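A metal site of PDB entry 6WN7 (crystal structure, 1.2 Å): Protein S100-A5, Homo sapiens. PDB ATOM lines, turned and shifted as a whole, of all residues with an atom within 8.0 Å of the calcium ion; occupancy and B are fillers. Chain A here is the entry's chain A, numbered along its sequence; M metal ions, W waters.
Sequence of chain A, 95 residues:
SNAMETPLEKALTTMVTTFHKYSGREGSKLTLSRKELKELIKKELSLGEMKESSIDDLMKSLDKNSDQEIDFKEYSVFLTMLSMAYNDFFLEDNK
The side-chain carboxylate of Glu 36 lies close to the backbone NH of Arg 25.
OE2 of Glu 69 sits at hydrogen-bond distance from OG1 of Thr 31 (2.9 Å).
The side-chain hydroxyl (OG) of Ser 28 is in hydrogen-bond range of the backbone NH (N) of Leu 30.
The backbone NH (N) of Glu 36 sits at hydrogen-bond distance from the side-chain hydroxyl (OG) of Ser 33, at 2.9 Å.
The side-chain carboxylate of Glu 26 sits at hydrogen-bond distance from the side-chain hydroxyl of Ser 33.
The side-chain hydroxyl (OG) of Ser 23 sits at hydrogen-bond distance from the backbone carbonyl oxygen (O) of Lys 29 (2.4 Å).
Within 4 Å of the calcium ion: Ser 23, Glu 26, Ser 28, Thr 31 and Glu 36.
The nearest printed residue that does not touch the calcium ion is Gly 27 (4.1 Å).
Water W1 binds the calcium ion (2.1 Å).
The calcium ion is bound by O of Ser 23 (2.2 Å).
The backbone carbonyl oxygen (O) of Ser 28 binds the calcium ion (2.3 Å).
The calcium ion is bound by O of Glu 26 (2.3 Å).
The calcium ion is bound by OE1 of Glu 36, at 2.3 Å.
The calcium ion is bound by the backbone carbonyl oxygen (O) of Thr 31 (2.5 Å).
The side-chain carboxylate (OE2) of Glu 36 is bound to the calcium ion, at 2.6 Å.
Water W1 lies within hydrogen-bond range of the side-chain carboxylate of Glu 69 and the side-chain hydroxyl of Thr 31.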
ATOM      1  N   PHE A  19     -16.757 -31.361   0.250  1.00  0.00           N
ATOM      2  CA  PHE A  19     -17.890 -30.500   0.615  1.00  0.00           C
ATOM      3  C   PHE A  19     -18.023 -30.413   2.128  1.00  0.00           C
ATOM      4  O   PHE A  19     -18.091 -29.324   2.692  1.00  0.00           O
ATOM      5  CB  PHE A  19     -19.163 -31.067   0.015  1.00  0.00           C
ATOM      6  CG  PHE A  19     -20.420 -30.350   0.427  1.00  0.00           C
ATOM      7  CD1 PHE A  19     -20.863 -29.271  -0.277  1.00  0.00           C
ATOM      8  CD2 PHE A  19     -21.173 -30.783   1.497  1.00  0.00           C
ATOM      9  CE1 PHE A  19     -21.984 -28.631   0.088  1.00  0.00           C
ATOM     10  CE2 PHE A  19     -22.328 -30.142   1.862  1.00  0.00           C
ATOM     11  CZ  PHE A  19     -22.717 -29.064   1.150  1.00  0.00           C
ATOM     12  N   HIS A  20     -18.093 -31.565   2.810  1.00  0.00           N
ATOM     13  CA  HIS A  20     -18.363 -31.573   4.243  1.00  0.00           C
ATOM     14  C   HIS A  20     -17.185 -31.060   5.047  1.00  0.00           C
ATOM     15  O   HIS A  20     -17.377 -30.556   6.149  1.00  0.00           O
ATOM     16  CB  HIS A  20     -18.795 -32.975   4.654  1.00  0.00           C
ATOM     17  CG  HIS A  20     -20.106 -33.402   4.067  1.00  0.00           C
ATOM     18  ND1 HIS A  20     -21.315 -32.986   4.576  1.00  0.00           N
ATOM     19  CD2 HIS A  20     -20.398 -34.177   3.008  1.00  0.00           C
ATOM     20  CE1 HIS A  20     -22.295 -33.506   3.856  1.00  0.00           C
ATOM     21  NE2 HIS A  20     -21.764 -34.241   2.897  1.00  0.00           N
ATOM     22  N   TYR A  22     -15.618 -28.377   4.391  1.00  0.00           N
ATOM     23  CA  TYR A  22     -15.753 -26.929   4.449  1.00  0.00           C
ATOM     24  C   TYR A  22     -17.145 -26.455   4.867  1.00  0.00           C
ATOM     25  O   TYR A  22     -17.269 -25.318   5.311  1.00  0.00           O
ATOM     26  CB  TYR A  22     -15.381 -26.317   3.089  1.00  0.00           C
ATOM     27  CG  TYR A  22     -13.900 -26.468   2.795  1.00  0.00           C
ATOM     28  CD1 TYR A  22     -12.986 -25.561   3.287  1.00  0.00           C
ATOM     29  CD2 TYR A  22     -13.413 -27.534   2.040  1.00  0.00           C
ATOM     30  CE1 TYR A  22     -11.646 -25.691   3.047  1.00  0.00           C
ATOM     31  CE2 TYR A  22     -12.056 -27.666   1.770  1.00  0.00           C
ATOM     32  CZ  TYR A  22     -11.182 -26.735   2.290  1.00  0.00           C
ATOM     33  OH  TYR A  22      -9.821 -26.846   2.055  1.00  0.00           O
ATOM     34  N   SER A  23     -18.177 -27.279   4.752  1.00  0.00           N
ATOM     35  CA  SER A  23     -19.516 -26.846   5.124  1.00  0.00           C
ATOM     36  C   SER A  23     -19.698 -26.766   6.634  1.00  0.00           C
ATOM     37  O   SER A  23     -20.681 -26.186   7.096  1.00  0.00           O
ATOM     38  CB  SER A  23     -20.579 -27.720   4.469  1.00  0.00           C
ATOM     39  OG  SER A  23     -20.674 -28.991   5.067  1.00  0.00           O
ATOM     40  N   GLY A  24     -18.772 -27.313   7.401  1.00  0.00           N
ATOM     41  CA  GLY A  24     -18.981 -27.378   8.828  1.00  0.00           C
ATOM     42  C   GLY A  24     -18.235 -26.338   9.623  1.00  0.00           C
ATOM     43  O   GLY A  24     -18.027 -26.511  10.832  1.00  0.00           O
ATOM     44  N   ARG A  25     -17.815 -25.259   8.965  1.00  0.00           N
ATOM     45  CA  ARG A  25     -17.050 -24.220   9.636  1.00  0.00           C
ATOM     46  C   ARG A  25     -17.945 -23.184  10.308  1.00  0.00           C
ATOM     47  O   ARG A  25     -17.641 -22.726  11.416  1.00  0.00           O
ATOM     48  CB  ARG A  25     -16.119 -23.523   8.640  1.00  0.00           C
ATOM     49  CG  ARG A  25     -15.154 -24.472   7.992  1.00  0.00           C
ATOM     50  CD  ARG A  25     -14.219 -23.792   7.014  1.00  0.00           C
ATOM     51  NE  ARG A  25     -13.030 -24.632   6.853  1.00  0.00           N
ATOM     52  CZ  ARG A  25     -11.839 -24.204   6.471  1.00  0.00           C
ATOM     53  NH1 ARG A  25     -11.652 -22.917   6.208  1.00  0.00           N
ATOM     54  NH2 ARG A  25     -10.839 -25.075   6.372  1.00  0.00           N
ATOM     55  N   GLU A  26     -19.023 -22.785   9.660  1.00  0.00           N
ATOM     56  CA  GLU A  26     -19.980 -21.875  10.254  1.00  0.00           C
ATOM     57  C   GLU A  26     -21.360 -22.310   9.803  1.00  0.00           C
ATOM     58  O   GLU A  26     -21.513 -23.083   8.856  1.00  0.00           O
ATOM     59  CB  GLU A  26     -19.679 -20.422   9.854  1.00  0.00           C
ATOM     60  CG  GLU A  26     -19.979 -20.061   8.385  1.00  0.00           C
ATOM     61  CD  GLU A  26     -19.560 -18.622   7.983  1.00  0.00           C
ATOM     62  OE1 GLU A  26     -19.565 -17.693   8.829  1.00  0.00           O
ATOM     63  OE2 GLU A  26     -19.227 -18.436   6.803  1.00  0.00           O
ATOM     64  N   GLY A  27     -22.356 -21.836  10.522  1.00  0.00           N
ATOM     65  CA  GLY A  27     -23.693 -22.104  10.101  1.00  0.00           C
ATOM     66  C   GLY A  27     -24.043 -23.575  10.152  1.00  0.00           C
ATOM     67  O   GLY A  27     -23.493 -24.347  10.910  1.00  0.00           O
ATOM     68  N   SER A  28     -25.030 -23.930   9.328  1.00  0.00           N
ATOM     69  CA  SER A  28     -25.320 -25.332   9.098  1.00  0.00           C
ATOM     70  C   SER A  28     -24.062 -26.051   8.605  1.00  0.00           C
ATOM     71  O   SER A  28     -23.307 -25.516   7.789  1.00  0.00           O
ATOM     72  CB  SER A  28     -26.401 -25.486   8.032  1.00  0.00           C
ATOM     73  OG  SER A  28     -26.568 -26.840   7.686  1.00  0.00           O
ATOM     74  N   LYS A  29     -23.843 -27.259   9.102  1.00  0.00           N
ATOM     75  CA  LYS A  29     -22.812 -28.122   8.552  1.00  0.00           C
ATOM     76  C   LYS A  29     -23.263 -28.807   7.271  1.00  0.00           C
ATOM     77  O   LYS A  29     -22.452 -29.483   6.627  1.00  0.00           O
ATOM     78  CB  LYS A  29     -22.381 -29.131   9.625  1.00  0.00           C
ATOM     79  N   LEU A  30     -24.516 -28.629   6.868  1.00  0.00           N
ATOM     80  CA  LEU A  30     -25.018 -29.229   5.646  1.00  0.00           C
ATOM     81  C   LEU A  30     -24.850 -28.337   4.422  1.00  0.00           C
ATOM     82  O   LEU A  30     -25.108 -28.789   3.295  1.00  0.00           O
ATOM     83  CB  LEU A  30     -26.511 -29.508   5.783  1.00  0.00           C
ATOM     84  CG  LEU A  30     -26.903 -30.743   6.589  1.00  0.00           C
ATOM     85  CD1 LEU A  30     -28.365 -31.032   6.344  1.00  0.00           C
ATOM     86  CD2 LEU A  30     -26.068 -31.921   6.222  1.00  0.00           C
ATOM     87  N   THR A  31     -24.454 -27.098   4.611  1.00  0.00           N
ATOM     88  CA  THR A  31     -24.393 -26.156   3.508  1.00  0.00           C
ATOM     89  C   THR A  31     -23.140 -25.318   3.616  1.00  0.00           C
ATOM     90  O   THR A  31     -22.583 -25.131   4.694  1.00  0.00           O
ATOM     91  CB  THR A  31     -25.607 -25.235   3.485  1.00  0.00           C
ATOM     92  OG1 THR A  31     -25.687 -24.547   4.748  1.00  0.00           O
ATOM     93  CG2 THR A  31     -26.872 -26.021   3.236  1.00  0.00           C
ATOM     94  N   LEU A  32     -22.732 -24.791   2.462  1.00  0.00           N
ATOM     95  CA  LEU A  32     -21.643 -23.830   2.358  1.00  0.00           C
ATOM     96  C   LEU A  32     -22.216 -22.412   2.275  1.00  0.00           C
ATOM     97  O   LEU A  32     -23.021 -22.112   1.386  1.00  0.00           O
ATOM     98  CB  LEU A  32     -20.833 -24.106   1.102  1.00  0.00           C
ATOM     99  CG  LEU A  32     -20.187 -25.474   0.923  1.00  0.00           C
ATOM    100  CD1 LEU A  32     -20.005 -25.744  -0.528  1.00  0.00           C
ATOM    101  CD2 LEU A  32     -18.884 -25.510   1.613  1.00  0.00           C
ATOM    102  N   SER A  33     -21.778 -21.566   3.209  1.00  0.00           N
ATOM    103  CA  SER A  33     -21.872 -20.128   3.068  1.00  0.00           C
ATOM    104  C   SER A  33     -20.938 -19.643   1.965  1.00  0.00           C
ATOM    105  O   SER A  33     -20.071 -20.378   1.481  1.00  0.00           O
ATOM    106  CB  SER A  33     -21.420 -19.470   4.385  1.00  0.00           C
ATOM    107  OG  SER A  33     -20.029 -19.585   4.530  1.00  0.00           O
ATOM    108  N   ARG A  34     -21.079 -18.357   1.599  1.00  0.00           N
ATOM    109  CA  ARG A  34     -20.158 -17.790   0.612  1.00  0.00           C
ATOM    110  C   ARG A  34     -18.728 -17.846   1.125  1.00  0.00           C
ATOM    111  O   ARG A  34     -17.809 -18.154   0.375  1.00  0.00           O
ATOM    112  CB  ARG A  34     -20.537 -16.354   0.260  1.00  0.00           C
ATOM    113  CG  ARG A  34     -19.688 -15.747  -0.850  1.00  0.00           C
ATOM    114  CD  ARG A  34     -20.422 -14.652  -1.607  1.00  0.00           C
ATOM    115  NE  ARG A  34     -19.967 -13.315  -1.230  1.00  0.00           N
ATOM    116  CZ  ARG A  34     -19.248 -12.507  -2.004  1.00  0.00           C
ATOM    117  NH1 ARG A  34     -18.873 -12.872  -3.219  1.00  0.00           N
ATOM    118  NH2 ARG A  34     -18.899 -11.305  -1.554  1.00  0.00           N
ATOM    119  N   GLU A  36     -17.502 -20.047   3.217  1.00  0.00           N
ATOM    120  CA  GLU A  36     -17.109 -21.445   3.133  1.00  0.00           C
ATOM    121  C   GLU A  36     -16.822 -21.867   1.697  1.00  0.00           C
ATOM    122  O   GLU A  36     -15.800 -22.475   1.411  1.00  0.00           O
ATOM    123  CB  GLU A  36     -18.181 -22.336   3.761  1.00  0.00           C
ATOM    124  CG  GLU A  36     -18.215 -22.255   5.274  1.00  0.00           C
ATOM    125  CD  GLU A  36     -19.345 -23.033   5.879  1.00  0.00           C
ATOM    126  OE1 GLU A  36     -20.389 -23.160   5.209  1.00  0.00           O
ATOM    127  OE2 GLU A  36     -19.214 -23.520   7.026  1.00  0.00           O
ATOM    128  N   LEU A  37     -17.714 -21.527   0.773  1.00  0.00           N
ATOM    129  CA  LEU A  37     -17.432 -21.788  -0.636  1.00  0.00           C
ATOM    130  C   LEU A  37     -16.072 -21.218  -1.057  1.00  0.00           C
ATOM    131  O   LEU A  37     -15.256 -21.913  -1.670  1.00  0.00           O
ATOM    132  CB  LEU A  37     -18.534 -21.166  -1.504  1.00  0.00           C
ATOM    133  CG  LEU A  37     -18.336 -21.280  -3.015  1.00  0.00           C
ATOM    134  CD1 LEU A  37     -18.011 -22.719  -3.418  1.00  0.00           C
ATOM    135  CD2 LEU A  37     -19.548 -20.788  -3.766  1.00  0.00           C
ATOM    136  N   GLU A  69     -27.294 -20.207   0.718  1.00  0.00           N
ATOM    137  CA  GLU A  69     -26.398 -21.285   1.125  1.00  0.00           C
ATOM    138  C   GLU A  69     -26.295 -22.285  -0.015  1.00  0.00           C
ATOM    139  O   GLU A  69     -27.260 -22.487  -0.746  1.00  0.00           O
ATOM    140  CB  GLU A  69     -26.965 -22.044   2.325  1.00  0.00           C
ATOM    141  CG  GLU A  69     -27.254 -21.184   3.555  1.00  0.00           C
ATOM    142  CD  GLU A  69     -26.079 -21.106   4.507  1.00  0.00           C
ATOM    143  OE1 GLU A  69     -26.159 -20.333   5.493  1.00  0.00           O
ATOM    144  OE2 GLU A  69     -25.070 -21.798   4.280  1.00  0.00           O
ATOM    145  N   ILE A  70     -25.145 -22.922  -0.145  1.00  0.00           N
ATOM    146  CA  ILE A  70     -24.957 -23.963  -1.154  1.00  0.00           C
ATOM    147  C   ILE A  70     -25.021 -25.326  -0.463  1.00  0.00           C
ATOM    148  O   ILE A  70     -24.159 -25.653   0.347  1.00  0.00           O
ATOM    149  CB  ILE A  70     -23.637 -23.771  -1.925  1.00  0.00           C
ATOM    150  CG1 ILE A  70     -23.569 -22.372  -2.541  1.00  0.00           C
ATOM    151  CG2 ILE A  70     -23.478 -24.801  -3.035  1.00  0.00           C
ATOM    152  CD1 ILE A  70     -24.813 -21.989  -3.285  1.00  0.00           C
HETATM  153 CA    CA M   1     -21.674 -24.232   6.853  1.00  0.00          CA
HETATM  154  O   HOH W   1     -23.252 -22.939   6.225  1.00  0.00           O
